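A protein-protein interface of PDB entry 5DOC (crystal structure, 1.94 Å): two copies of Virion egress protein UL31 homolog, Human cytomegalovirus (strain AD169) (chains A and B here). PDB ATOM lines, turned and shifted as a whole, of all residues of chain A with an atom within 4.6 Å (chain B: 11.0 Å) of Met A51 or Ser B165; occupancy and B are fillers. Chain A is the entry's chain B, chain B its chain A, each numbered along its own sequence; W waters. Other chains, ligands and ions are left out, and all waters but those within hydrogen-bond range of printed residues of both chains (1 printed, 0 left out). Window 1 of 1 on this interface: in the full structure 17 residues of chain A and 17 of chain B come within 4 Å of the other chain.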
ATOM      1  N   ALA A  47     -13.616 -35.010  -8.495  1.00  0.00           N
ATOM      2  CA  ALA A  47     -14.171 -33.650  -8.573  1.00  0.00           C
ATOM      3  C   ALA A  47     -15.705 -33.707  -8.500  1.00  0.00           C
ATOM      4  O   ALA A  47     -16.301 -32.848  -7.928  1.00  0.00           O
ATOM      5  CB  ALA A  47     -13.741 -32.958  -9.863  1.00  0.00           C
ATOM      6  N   SER A  48     -16.320 -34.732  -9.077  1.00  0.00           N
ATOM      7  CA  SER A  48     -17.800 -34.905  -8.936  1.00  0.00           C
ATOM      8  C   SER A  48     -18.198 -35.138  -7.476  1.00  0.00           C
ATOM      9  O   SER A  48     -19.155 -34.520  -6.978  1.00  0.00           O
ATOM     10  CB  SER A  48     -18.296 -36.035  -9.811  1.00  0.00           C
ATOM     11  OG  SER A  48     -18.196 -35.624 -11.142  1.00  0.00           O
ATOM     12  N   ASP A  49     -17.479 -36.039  -6.781  1.00  0.00           N
ATOM     13  CA  ASP A  49     -17.754 -36.240  -5.361  1.00  0.00           C
ATOM     14  C   ASP A  49     -17.599 -34.920  -4.593  1.00  0.00           C
ATOM     15  O   ASP A  49     -18.375 -34.624  -3.684  1.00  0.00           O
ATOM     16  CB  ASP A  49     -16.806 -37.254  -4.727  1.00  0.00           C
ATOM     17  CG  ASP A  49     -16.954 -38.658  -5.290  1.00  0.00           C
ATOM     18  OD1 ASP A  49     -18.119 -39.085  -5.573  1.00  0.00           O
ATOM     19  OD2 ASP A  49     -15.885 -39.336  -5.427  1.00  0.00           O
ATOM     20  N   ALA A  50     -16.585 -34.130  -4.962  1.00  0.00           N
ATOM     21  CA  ALA A  50     -16.323 -32.904  -4.270  1.00  0.00           C
ATOM     22  C   ALA A  50     -17.448 -31.846  -4.545  1.00  0.00           C
ATOM     23  O   ALA A  50     -17.768 -31.050  -3.670  1.00  0.00           O
ATOM     24  CB  ALA A  50     -14.945 -32.367  -4.633  1.00  0.00           C
ATOM     25  N   MET A  51     -18.046 -31.884  -5.718  1.00  0.00           N
ATOM     26  CA  MET A  51     -19.205 -31.029  -6.010  1.00  0.00           C
ATOM     27  C   MET A  51     -20.422 -31.456  -5.172  1.00  0.00           C
ATOM     28  O   MET A  51     -21.155 -30.620  -4.683  1.00  0.00           O
ATOM     29  CB  MET A  51     -19.527 -31.066  -7.514  1.00  0.00           C
ATOM     30  CG  MET A  51     -20.789 -30.290  -7.925  1.00  0.00           C
ATOM     31  SD  MET A  51     -20.642 -28.522  -7.543  1.00  0.00           S
ATOM     32  CE  MET A  51     -19.766 -27.976  -8.992  1.00  0.00           C
ATOM     33  N   VAL A  52     -20.619 -32.758  -5.024  1.00  0.00           N
ATOM     34  CA  VAL A  52     -21.728 -33.258  -4.182  1.00  0.00           C
ATOM     35  C   VAL A  52     -21.472 -32.797  -2.763  1.00  0.00           C
ATOM     36  O   VAL A  52     -22.387 -32.333  -2.133  1.00  0.00           O
ATOM     37  CB  VAL A  52     -21.920 -34.788  -4.263  1.00  0.00           C
ATOM     38  CG1 VAL A  52     -22.957 -35.251  -3.253  1.00  0.00           C
ATOM     39  CG2 VAL A  52     -22.319 -35.173  -5.661  1.00  0.00           C
ATOM     40  N   ALA A  53     -20.213 -32.844  -2.303  1.00  0.00           N
ATOM     41  CA  ALA A  53     -19.861 -32.325  -0.973  1.00  0.00           C
ATOM     42  C   ALA A  53     -20.091 -30.822  -0.865  1.00  0.00           C
ATOM     43  O   ALA A  53     -20.522 -30.329   0.185  1.00  0.00           O
ATOM     44  CB  ALA A  53     -18.425 -32.664  -0.594  1.00  0.00           C
ATOM     45  N   PHE A  54     -19.765 -30.099  -1.939  1.00  0.00           N
ATOM     46  CA  PHE A  54     -20.031 -28.668  -1.975  1.00  0.00           C
ATOM     47  C   PHE A  54     -21.555 -28.444  -1.785  1.00  0.00           C
ATOM     48  O   PHE A  54     -21.976 -27.634  -0.972  1.00  0.00           O
ATOM     49  CB  PHE A  54     -19.565 -28.034  -3.291  1.00  0.00           C
ATOM     50  CG  PHE A  54     -20.058 -26.628  -3.482  1.00  0.00           C
ATOM     51  CD1 PHE A  54     -19.390 -25.576  -2.907  1.00  0.00           C
ATOM     52  CD2 PHE A  54     -21.231 -26.365  -4.218  1.00  0.00           C
ATOM     53  CE1 PHE A  54     -19.847 -24.275  -3.077  1.00  0.00           C
ATOM     54  CE2 PHE A  54     -21.688 -25.054  -4.390  1.00  0.00           C
ATOM     55  CZ  PHE A  54     -20.958 -23.997  -3.866  1.00  0.00           C
ATOM     56  N   ILE A  55     -22.345 -29.156  -2.539  1.00  0.00           N
ATOM     57  CA  ILE A  55     -23.811 -29.073  -2.415  1.00  0.00           C
ATOM     58  C   ILE A  55     -24.289 -29.383  -0.992  1.00  0.00           C
ATOM     59  O   ILE A  55     -25.234 -28.749  -0.514  1.00  0.00           O
ATOM     60  CB  ILE A  55     -24.503 -29.923  -3.481  1.00  0.00           C
ATOM     61  CG1 ILE A  55     -24.307 -29.240  -4.849  1.00  0.00           C
ATOM     62  CG2 ILE A  55     -25.987 -30.154  -3.188  1.00  0.00           C
ATOM     63  CD1 ILE A  55     -24.553 -30.140  -6.033  1.00  0.00           C
ATOM     64  N   PRO A  85     -17.860 -22.952  -6.502  1.00  0.00           N
ATOM     65  CA  PRO A  85     -17.635 -24.340  -6.096  1.00  0.00           C
ATOM     66  C   PRO A  85     -16.201 -24.860  -6.151  1.00  0.00           C
ATOM     67  O   PRO A  85     -15.833 -25.595  -5.258  1.00  0.00           O
ATOM     68  CB  PRO A  85     -18.541 -25.136  -7.026  1.00  0.00           C
ATOM     69  CG  PRO A  85     -19.631 -24.156  -7.402  1.00  0.00           C
ATOM     70  CD  PRO A  85     -18.963 -22.829  -7.478  1.00  0.00           C
ATOM     71  N   PRO A  86     -15.376 -24.467  -7.162  1.00  0.00           N
ATOM     72  CA  PRO A  86     -14.004 -24.985  -7.202  1.00  0.00           C
ATOM     73  C   PRO A  86     -13.097 -24.732  -5.991  1.00  0.00           C
ATOM     74  O   PRO A  86     -12.232 -25.570  -5.711  1.00  0.00           O
ATOM     75  CB  PRO A  86     -13.411 -24.329  -8.464  1.00  0.00           C
ATOM     76  CG  PRO A  86     -14.595 -24.103  -9.352  1.00  0.00           C
ATOM     77  CD  PRO A  86     -15.660 -23.648  -8.356  1.00  0.00           C
ATOM     78  N   GLN A  89     -14.225 -27.380  -3.701  1.00  0.00           N
ATOM     79  CA  GLN A  89     -13.871 -28.663  -4.316  1.00  0.00           C
ATOM     80  C   GLN A  89     -12.387 -28.972  -4.118  1.00  0.00           C
ATOM     81  O   GLN A  89     -12.021 -30.091  -3.724  1.00  0.00           O
ATOM     82  CB  GLN A  89     -14.219 -28.663  -5.793  1.00  0.00           C
ATOM     83  CG  GLN A  89     -15.697 -28.776  -6.090  1.00  0.00           C
ATOM     84  CD  GLN A  89     -15.926 -28.800  -7.577  1.00  0.00           C
ATOM     85  OE1 GLN A  89     -15.979 -29.887  -8.229  1.00  0.00           O
ATOM     86  NE2 GLN A  89     -16.134 -27.640  -8.126  1.00  0.00           N
ATOM     87  N   THR A 135      -9.515 -30.874 -12.960  1.00  0.00           N
ATOM     88  CA  THR A 135     -10.939 -30.866 -13.373  1.00  0.00           C
ATOM     89  C   THR A 135     -11.715 -29.718 -12.703  1.00  0.00           C
ATOM     90  O   THR A 135     -12.437 -28.966 -13.378  1.00  0.00           O
ATOM     91  CB  THR A 135     -11.621 -32.215 -13.069  1.00  0.00           C
ATOM     92  OG1 THR A 135     -10.989 -33.193 -13.847  1.00  0.00           O
ATOM     93  CG2 THR A 135     -13.092 -32.250 -13.421  1.00  0.00           C
ATOM     94  N   ALA A 136     -11.570 -29.592 -11.386  1.00  0.00           N
ATOM     95  CA  ALA A 136     -12.266 -28.560 -10.656  1.00  0.00           C
ATOM     96  C   ALA A 136     -11.813 -27.153 -11.065  1.00  0.00           C
ATOM     97  O   ALA A 136     -12.616 -26.231 -11.062  1.00  0.00           O
ATOM     98  CB  ALA A 136     -12.083 -28.743  -9.164  1.00  0.00           C
ATOM     99  N   ALA B  47     -32.362 -27.002  -8.336  1.00  0.00           N
ATOM    100  CA  ALA B  47     -31.241 -26.987  -9.290  1.00  0.00           C
ATOM    101  C   ALA B  47     -30.076 -27.837  -8.722  1.00  0.00           C
ATOM    102  O   ALA B  47     -29.420 -28.500  -9.479  1.00  0.00           O
ATOM    103  CB  ALA B  47     -30.749 -25.585  -9.564  1.00  0.00           C
ATOM    104  N   SER B  48     -29.852 -27.803  -7.402  1.00  0.00           N
ATOM    105  CA  SER B  48     -28.843 -28.672  -6.784  1.00  0.00           C
ATOM    106  C   SER B  48     -29.150 -30.140  -6.984  1.00  0.00           C
ATOM    107  O   SER B  48     -28.273 -30.915  -7.390  1.00  0.00           O
ATOM    108  CB  SER B  48     -28.705 -28.373  -5.306  1.00  0.00           C
ATOM    109  OG  SER B  48     -28.101 -27.119  -5.169  1.00  0.00           O
ATOM    110  N   ASP B  49     -30.395 -30.546  -6.735  1.00  0.00           N
ATOM    111  CA  ASP B  49     -30.789 -31.911  -7.014  1.00  0.00           C
ATOM    112  C   ASP B  49     -30.487 -32.262  -8.483  1.00  0.00           C
ATOM    113  O   ASP B  49     -30.040 -33.350  -8.796  1.00  0.00           O
ATOM    114  CB  ASP B  49     -32.270 -32.157  -6.761  1.00  0.00           C
ATOM    115  CG  ASP B  49     -32.671 -32.020  -5.277  1.00  0.00           C
ATOM    116  OD1 ASP B  49     -31.883 -32.442  -4.382  1.00  0.00           O
ATOM    117  OD2 ASP B  49     -33.792 -31.530  -5.050  1.00  0.00           O
ATOM    118  N   ALA B  50     -30.799 -31.331  -9.386  1.00  0.00           N
ATOM    119  CA  ALA B  50     -30.679 -31.597 -10.798  1.00  0.00           C
ATOM    120  C   ALA B  50     -29.190 -31.726 -11.190  1.00  0.00           C
ATOM    121  O   ALA B  50     -28.855 -32.508 -12.091  1.00  0.00           O
ATOM    122  CB  ALA B  50     -31.424 -30.500 -11.619  1.00  0.00           C
ATOM    123  N   MET B  51     -28.316 -31.006 -10.493  1.00  0.00           N
ATOM    124  CA  MET B  51     -26.867 -31.131 -10.684  1.00  0.00           C
ATOM    125  C   MET B  51     -26.355 -32.505 -10.175  1.00  0.00           C
ATOM    126  O   MET B  51     -25.556 -33.147 -10.839  1.00  0.00           O
ATOM    127  CB  MET B  51     -26.115 -30.009  -9.995  1.00  0.00           C
ATOM    128  CG  MET B  51     -24.606 -30.116 -10.031  1.00  0.00           C
ATOM    129  SD  MET B  51     -23.924 -30.113 -11.725  1.00  0.00           S
ATOM    130  CE  MET B  51     -23.848 -28.362 -12.014  1.00  0.00           C
ATOM    131  N   VAL B  52     -26.872 -32.964  -9.037  1.00  0.00           N
ATOM    132  CA  VAL B  52     -26.537 -34.314  -8.546  1.00  0.00           C
ATOM    133  C   VAL B  52     -26.979 -35.367  -9.558  1.00  0.00           C
ATOM    134  O   VAL B  52     -26.237 -36.272  -9.845  1.00  0.00           O
ATOM    135  CB  VAL B  52     -27.079 -34.598  -7.142  1.00  0.00           C
ATOM    136  CG1 VAL B  52     -26.779 -36.015  -6.743  1.00  0.00           C
ATOM    137  CG2 VAL B  52     -26.471 -33.654  -6.121  1.00  0.00           C
ATOM    138  N   ALA B  53     -28.181 -35.214 -10.119  1.00  0.00           N
ATOM    139  CA  ALA B  53     -28.650 -36.117 -11.158  1.00  0.00           C
ATOM    140  C   ALA B  53     -27.754 -36.050 -12.406  1.00  0.00           C
ATOM    141  O   ALA B  53     -27.567 -37.080 -13.072  1.00  0.00           O
ATOM    142  CB  ALA B  53     -30.113 -35.821 -11.543  1.00  0.00           C
ATOM    143  N   PHE B  54     -27.294 -34.843 -12.763  1.00  0.00           N
ATOM    144  CA  PHE B  54     -26.396 -34.668 -13.901  1.00  0.00           C
ATOM    145  C   PHE B  54     -25.128 -35.482 -13.606  1.00  0.00           C
ATOM    146  O   PHE B  54     -24.652 -36.249 -14.441  1.00  0.00           O
ATOM    147  CB  PHE B  54     -26.051 -33.183 -14.158  1.00  0.00           C
ATOM    148  CG  PHE B  54     -24.909 -32.984 -15.115  1.00  0.00           C
ATOM    149  CD1 PHE B  54     -25.129 -32.995 -16.484  1.00  0.00           C
ATOM    150  CD2 PHE B  54     -23.589 -32.874 -14.656  1.00  0.00           C
ATOM    151  CE1 PHE B  54     -24.070 -32.851 -17.389  1.00  0.00           C
ATOM    152  CE2 PHE B  54     -22.522 -32.757 -15.560  1.00  0.00           C
ATOM    153  CZ  PHE B  54     -22.771 -32.712 -16.932  1.00  0.00           C
ATOM    154  N   ILE B  55     -24.598 -35.317 -12.418  1.00  0.00           N
ATOM    155  CA  ILE B  55     -23.390 -36.066 -12.006  1.00  0.00           C
ATOM    156  C   ILE B  55     -23.591 -37.577 -12.051  1.00  0.00           C
ATOM    157  O   ILE B  55     -22.695 -38.302 -12.457  1.00  0.00           O
ATOM    158  CB  ILE B  55     -22.938 -35.607 -10.627  1.00  0.00           C
ATOM    159  CG1 ILE B  55     -22.327 -34.206 -10.811  1.00  0.00           C
ATOM    160  CG2 ILE B  55     -21.963 -36.611  -9.964  1.00  0.00           C
ATOM    161  CD1 ILE B  55     -22.159 -33.462  -9.523  1.00  0.00           C
ATOM    162  N   ASN B  56     -24.818 -38.025 -11.740  1.00  0.00           N
ATOM    163  CA  ASN B  56     -25.089 -39.430 -11.620  1.00  0.00           C
ATOM    164  C   ASN B  56     -25.742 -40.005 -12.886  1.00  0.00           C
ATOM    165  O   ASN B  56     -26.363 -41.087 -12.822  1.00  0.00           O
ATOM    166  CB  ASN B  56     -26.019 -39.673 -10.395  1.00  0.00           C
ATOM    167  CG  ASN B  56     -25.325 -39.469  -9.065  1.00  0.00           C
ATOM    168  OD1 ASN B  56     -25.961 -39.047  -8.104  1.00  0.00           O
ATOM    169  ND2 ASN B  56     -24.107 -39.795  -8.971  1.00  0.00           N
ATOM    170  N   SER B  81     -23.269 -31.982 -24.342  1.00  0.00           N
ATOM    171  CA  SER B  81     -24.117 -31.915 -23.152  1.00  0.00           C
ATOM    172  C   SER B  81     -23.292 -32.158 -21.888  1.00  0.00           C
ATOM    173  O   SER B  81     -23.564 -31.580 -20.820  1.00  0.00           O
ATOM    174  CB  SER B  81     -25.321 -32.900 -23.213  1.00  0.00           C
ATOM    175  OG  SER B  81     -24.945 -34.252 -22.886  1.00  0.00           O
ATOM    176  N   THR B  82     -22.270 -32.992 -21.993  1.00  0.00           N
ATOM    177  CA  THR B  82     -21.492 -33.293 -20.820  1.00  0.00           C
ATOM    178  C   THR B  82     -20.608 -32.110 -20.370  1.00  0.00           C
ATOM    179  O   THR B  82     -20.083 -32.140 -19.266  1.00  0.00           O
ATOM    180  CB  THR B  82     -20.591 -34.562 -20.990  1.00  0.00           C
ATOM    181  OG1 THR B  82     -19.607 -34.331 -22.004  1.00  0.00           O
ATOM    182  CG2 THR B  82     -21.398 -35.798 -21.376  1.00  0.00           C
ATOM    183  N   ASN B  83     -20.414 -31.107 -21.233  1.00  0.00           N
ATOM    184  CA  ASN B  83     -19.749 -29.857 -20.847  1.00  0.00           C
ATOM    185  C   ASN B  83     -20.690 -28.760 -20.396  1.00  0.00           C
ATOM    186  O   ASN B  83     -20.231 -27.722 -19.973  1.00  0.00           O
ATOM    187  CB  ASN B  83     -18.948 -29.300 -22.027  1.00  0.00           C
ATOM    188  CG  ASN B  83     -17.857 -30.235 -22.487  1.00  0.00           C
ATOM    189  OD1 ASN B  83     -17.484 -30.225 -23.663  1.00  0.00           O
ATOM    190  ND2 ASN B  83     -17.320 -31.015 -21.590  1.00  0.00           N
ATOM    191  N   GLN B  84     -22.002 -29.014 -20.470  1.00  0.00           N
ATOM    192  CA  GLN B  84     -23.020 -28.037 -20.176  1.00  0.00           C
ATOM    193  C   GLN B  84     -24.101 -28.636 -19.246  1.00  0.00           C
ATOM    194  O   GLN B  84     -25.209 -28.958 -19.698  1.00  0.00           O
ATOM    195  CB  GLN B  84     -23.671 -27.540 -21.488  1.00  0.00           C
ATOM    196  CG  GLN B  84     -22.785 -26.762 -22.440  1.00  0.00           C
ATOM    197  CD  GLN B  84     -23.514 -26.428 -23.737  1.00  0.00           C
ATOM    198  OE1 GLN B  84     -23.005 -26.648 -24.843  1.00  0.00           O
ATOM    199  NE2 GLN B  84     -24.729 -25.904 -23.610  1.00  0.00           N
ATOM    200  N   PRO B  85     -23.796 -28.753 -17.945  1.00  0.00           N
ATOM    201  CA  PRO B  85     -24.792 -29.251 -16.980  1.00  0.00           C
ATOM    202  C   PRO B  85     -26.171 -28.626 -17.048  1.00  0.00           C
ATOM    203  O   PRO B  85     -27.146 -29.321 -16.855  1.00  0.00           O
ATOM    204  CB  PRO B  85     -24.129 -29.016 -15.637  1.00  0.00           C
ATOM    205  CG  PRO B  85     -22.633 -29.064 -15.960  1.00  0.00           C
ATOM    206  CD  PRO B  85     -22.500 -28.470 -17.309  1.00  0.00           C
ATOM    207  N   PRO B  86     -26.273 -27.297 -17.283  1.00  0.00           N
ATOM    208  CA  PRO B  86     -27.596 -26.724 -17.321  1.00  0.00           C
ATOM    209  C   PRO B  86     -28.594 -27.280 -18.348  1.00  0.00           C
ATOM    210  O   PRO B  86     -29.794 -27.152 -18.120  1.00  0.00           O
ATOM    211  CB  PRO B  86     -27.312 -25.227 -17.606  1.00  0.00           C
ATOM    212  CG  PRO B  86     -25.966 -25.010 -17.033  1.00  0.00           C
ATOM    213  CD  PRO B  86     -25.235 -26.267 -17.433  1.00  0.00           C
ATOM    214  N   GLN B  89     -29.882 -30.111 -16.499  1.00  0.00           N
ATOM    215  CA  GLN B  89     -30.554 -29.599 -15.292  1.00  0.00           C
ATOM    216  C   GLN B  89     -31.925 -29.030 -15.611  1.00  0.00           C
ATOM    217  O   GLN B  89     -32.924 -29.399 -14.959  1.00  0.00           O
ATOM    218  CB  GLN B  89     -29.721 -28.551 -14.607  1.00  0.00           C
ATOM    219  CG  GLN B  89     -28.542 -29.059 -13.855  1.00  0.00           C
ATOM    220  CD  GLN B  89     -27.807 -27.907 -13.176  1.00  0.00           C
ATOM    221  OE1 GLN B  89     -28.064 -27.534 -11.996  1.00  0.00           O
ATOM    222  NE2 GLN B  89     -26.899 -27.341 -13.910  1.00  0.00           N
ATOM    223  N   ARG B 138     -28.489 -19.288 -15.046  1.00  0.00           N
ATOM    224  CA  ARG B 138     -27.881 -18.000 -14.715  1.00  0.00           C
ATOM    225  C   ARG B 138     -26.692 -17.659 -15.599  1.00  0.00           C
ATOM    226  O   ARG B 138     -25.750 -18.454 -15.756  1.00  0.00           O
ATOM    227  CB  ARG B 138     -27.434 -18.009 -13.244  1.00  0.00           C
ATOM    228  CG  ARG B 138     -26.942 -16.678 -12.680  1.00  0.00           C
ATOM    229  CD  ARG B 138     -26.963 -16.658 -11.144  1.00  0.00           C
ATOM    230  NE  ARG B 138     -25.908 -17.501 -10.543  1.00  0.00           N
ATOM    231  CZ  ARG B 138     -24.622 -17.147 -10.424  1.00  0.00           C
ATOM    232  NH1 ARG B 138     -24.198 -15.962 -10.855  1.00  0.00           N
ATOM    233  NH2 ARG B 138     -23.752 -17.980  -9.868  1.00  0.00           N
ATOM    234  N   ASP B 140     -25.393 -17.638 -18.537  1.00  0.00           N
ATOM    235  CA  ASP B 140     -24.960 -18.156 -19.828  1.00  0.00           C
ATOM    236  C   ASP B 140     -26.081 -18.648 -20.756  1.00  0.00           C
ATOM    237  O   ASP B 140     -25.804 -18.958 -21.926  1.00  0.00           O
ATOM    238  CB  ASP B 140     -23.913 -19.248 -19.626  1.00  0.00           C
ATOM    239  CG  ASP B 140     -22.654 -18.732 -18.954  1.00  0.00           C
ATOM    240  OD1 ASP B 140     -22.340 -17.526 -19.061  1.00  0.00           O
ATOM    241  OD2 ASP B 140     -21.998 -19.528 -18.295  1.00  0.00           O
ATOM    242  N   VAL B 161     -20.290 -21.118 -23.010  1.00  0.00           N
ATOM    243  CA  VAL B 161     -20.087 -22.325 -22.211  1.00  0.00           C
ATOM    244  C   VAL B 161     -18.956 -22.067 -21.245  1.00  0.00           C
ATOM    245  O   VAL B 161     -17.819 -22.011 -21.647  1.00  0.00           O
ATOM    246  CB  VAL B 161     -19.806 -23.530 -23.084  1.00  0.00           C
ATOM    247  CG1 VAL B 161     -19.557 -24.775 -22.203  1.00  0.00           C
ATOM    248  CG2 VAL B 161     -20.968 -23.762 -24.024  1.00  0.00           C
ATOM    249  N   SER B 162     -19.315 -21.805 -19.991  1.00  0.00           N
ATOM    250  CA  SER B 162     -18.344 -21.653 -18.899  1.00  0.00           C
ATOM    251  C   SER B 162     -17.816 -23.010 -18.462  1.00  0.00           C
ATOM    252  O   SER B 162     -18.499 -24.034 -18.595  1.00  0.00           O
ATOM    253  CB  SER B 162     -19.006 -21.046 -17.678  1.00  0.00           C
ATOM    254  OG  SER B 162     -19.508 -19.751 -17.928  1.00  0.00           O
ATOM    255  N   ALA B 163     -16.619 -22.992 -17.904  1.00  0.00           N
ATOM    256  CA  ALA B 163     -15.967 -24.208 -17.434  1.00  0.00           C
ATOM    257  C   ALA B 163     -16.879 -24.934 -16.487  1.00  0.00           C
ATOM    258  O   ALA B 163     -17.458 -24.308 -15.614  1.00  0.00           O
ATOM    259  CB  ALA B 163     -14.687 -23.830 -16.700  1.00  0.00           C
ATOM    260  N   SER B 164     -17.066 -26.237 -16.685  1.00  0.00           N
ATOM    261  CA  SER B 164     -17.746 -27.051 -15.697  1.00  0.00           C
ATOM    262  C   SER B 164     -16.685 -27.656 -14.787  1.00  0.00           C
ATOM    263  O   SER B 164     -15.650 -28.119 -15.266  1.00  0.00           O
ATOM    264  CB  SER B 164     -18.542 -28.159 -16.375  1.00  0.00           C
ATOM    265  OG  SER B 164     -19.153 -28.969 -15.405  1.00  0.00           O
ATOM    266  N   SER B 165     -16.936 -27.646 -13.483  1.00  0.00           N
ATOM    267  CA  SER B 165     -15.955 -28.163 -12.504  1.00  0.00           C
ATOM    268  C   SER B 165     -16.141 -29.652 -12.130  1.00  0.00           C
ATOM    269  O   SER B 165     -15.590 -30.136 -11.109  1.00  0.00           O
ATOM    270  CB  SER B 165     -15.973 -27.275 -11.268  1.00  0.00           C
ATOM    271  OG  SER B 165     -17.223 -27.388 -10.578  1.00  0.00           O
ATOM    272  N   VAL B 166     -16.906 -30.367 -12.960  1.00  0.00           N
ATOM    273  CA  VAL B 166     -17.067 -31.821 -12.822  1.00  0.00           C
ATOM    274  C   VAL B 166     -16.915 -32.486 -14.159  1.00  0.00           C
ATOM    275  O   VAL B 166     -17.051 -31.856 -15.161  1.00  0.00           O
ATOM    276  CB  VAL B 166     -18.435 -32.223 -12.232  1.00  0.00           C
ATOM    277  CG1 VAL B 166     -18.572 -31.635 -10.838  1.00  0.00           C
ATOM    278  CG2 VAL B 166     -19.566 -31.747 -13.132  1.00  0.00           C
ATOM    279  N   LYS B 167     -16.585 -33.755 -14.159  1.00  0.00           N
ATOM    280  CA  LYS B 167     -16.434 -34.473 -15.399  1.00  0.00           C
ATOM    281  C   LYS B 167     -17.347 -35.724 -15.365  1.00  0.00           C
ATOM    282  O   LYS B 167     -17.432 -36.416 -14.356  1.00  0.00           O
ATOM    283  CB  LYS B 167     -14.986 -34.858 -15.560  1.00  0.00           C
ATOM    284  CG  LYS B 167     -14.630 -35.639 -16.810  1.00  0.00           C
ATOM    285  CD  LYS B 167     -13.115 -35.732 -16.900  1.00  0.00           C
ATOM    286  CE  LYS B 167     -12.709 -36.511 -18.143  1.00  0.00           C
ATOM    287  NZ  LYS B 167     -12.786 -37.980 -17.868  1.00  0.00           N
ATOM    288  N   ILE B 168     -18.042 -35.954 -16.460  1.00  0.00           N
ATOM    289  CA  ILE B 168     -18.842 -37.140 -16.675  1.00  0.00           C
ATOM    290  C   ILE B 168     -18.027 -38.136 -17.495  1.00  0.00           C
ATOM    291  O   ILE B 168     -17.239 -37.723 -18.366  1.00  0.00           O
ATOM    292  CB  ILE B 168     -20.118 -36.733 -17.478  1.00  0.00           C
ATOM    293  CG1 ILE B 168     -20.976 -35.768 -16.660  1.00  0.00           C
ATOM    294  CG2 ILE B 168     -20.901 -37.934 -17.942  1.00  0.00           C
ATOM    295  CD1 ILE B 168     -21.153 -36.191 -15.213  1.00  0.00           C
HETATM  296  O   HOH W   1     -15.367 -35.476 -11.801  1.00  0.00           O
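NE2 of Gln A89 lies within hydrogen-bond range of OG of Ser B165, 2.7 Å away. The backbone carbonyl oxygen (O) of Lys B167 is in hydrogen-bond range of the side-chain hydroxyl (OG) of Ser A48 (3.4 Å).
The backbone carbonyl oxygen (O) of Ala A47 lies close to the side-chain amide oxygen (OE1) of Gln A89 (3.0 Å).
Among the printed residues, pairs that only touch across the chains: Met A51 with Ser B165 (3.1 Å), Met A51 with Val B166 (3.5 Å), Ala A136 with Ser B165 (3.5 Å), Ser A48 with Val B166 (3.6 Å), Ala A47 with Ser B165 (3.6 Å), Thr A135 with Ser B165 (3.7 Å), Ser A48 with Ile B55 (3.7 Å), Met A51 with Ile B55 (3.8 Å), Thr A135 with Ser B164 (3.8 Å), Thr A135 with Lys B167 (3.9 Å), Ile A55 with Ser B48 (3.9 Å), Ala A47 with Val B166 (3.9 Å), Thr A135 with Val B166 (3.9 Å), Pro A86 with Ser B165 (3.95 Å) and Ile A55 with Met B51 (3.998 Å).
Ala A47 touches just these residues of chain B: Ser B165 (3.6 Å) and Val B166 (3.9 Å). Printed residues of chain B within 4 Å of Met A51: Ile B55, Ser B165 and Val B166. No residue of chain B comes within 4 Å of Ala A53. No residue of chain B comes within 4 Å of Phe A54. Of the printed residues of chain B, Ile A55 touches Ser B48 (3.9 Å) and Met B51 (3.998 Å). Pro A85 touches none of the printed residues of chain B. Thr A135 touches just these residues of chain B: Ser B164 (3.8 Å), Ser B165 (3.7 Å), Val B166 (3.9 Å) and Lys B167 (3.9 Å). Ala A136 touches just one residue of chain B: Ser B165. Of the printed residues of chain A, Ser B48 touches Ile A55 (3.9 Å). Printed residues of chain A within 4 Å of Ser B165: Ala A47 (3.6 Å), Met A51 (3.1 Å), Pro A86 (3.95 Å), Gln A89 (2.7 Å), Thr A135 (3.7 Å) and Ala A136 (3.5 Å). The nearest residue of chain B that does not touch Met A51 is Met B51 (4.4 Å). The nearest printed residue of chain A that does not touch Ser B164 is Ala A136 (5.5 Å).
Of the 14 printed residues of chain A, 8 touch a printed residue of chain B. Printed residues of chain A that touch a printed residue of chain B: Ala A47, Ser A48, Met A51, Ile A55, Pro A86, Gln A89, Thr A135 and Ala A136. Among the printed residues, 17 pairs touch across the chains.
Ser A48 touches Ile B55, and with the chains exchanged Ile A55 touches Ser B48. Met A51 touches Ile B55, and with the chains exchanged Ile A55 touches Met B51.
Water W1 bridges the side-chain hydroxyl (OG) of Ser A48 (2.9 Å) and the backbone NH (N) of Lys B167 (3.2 Å).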
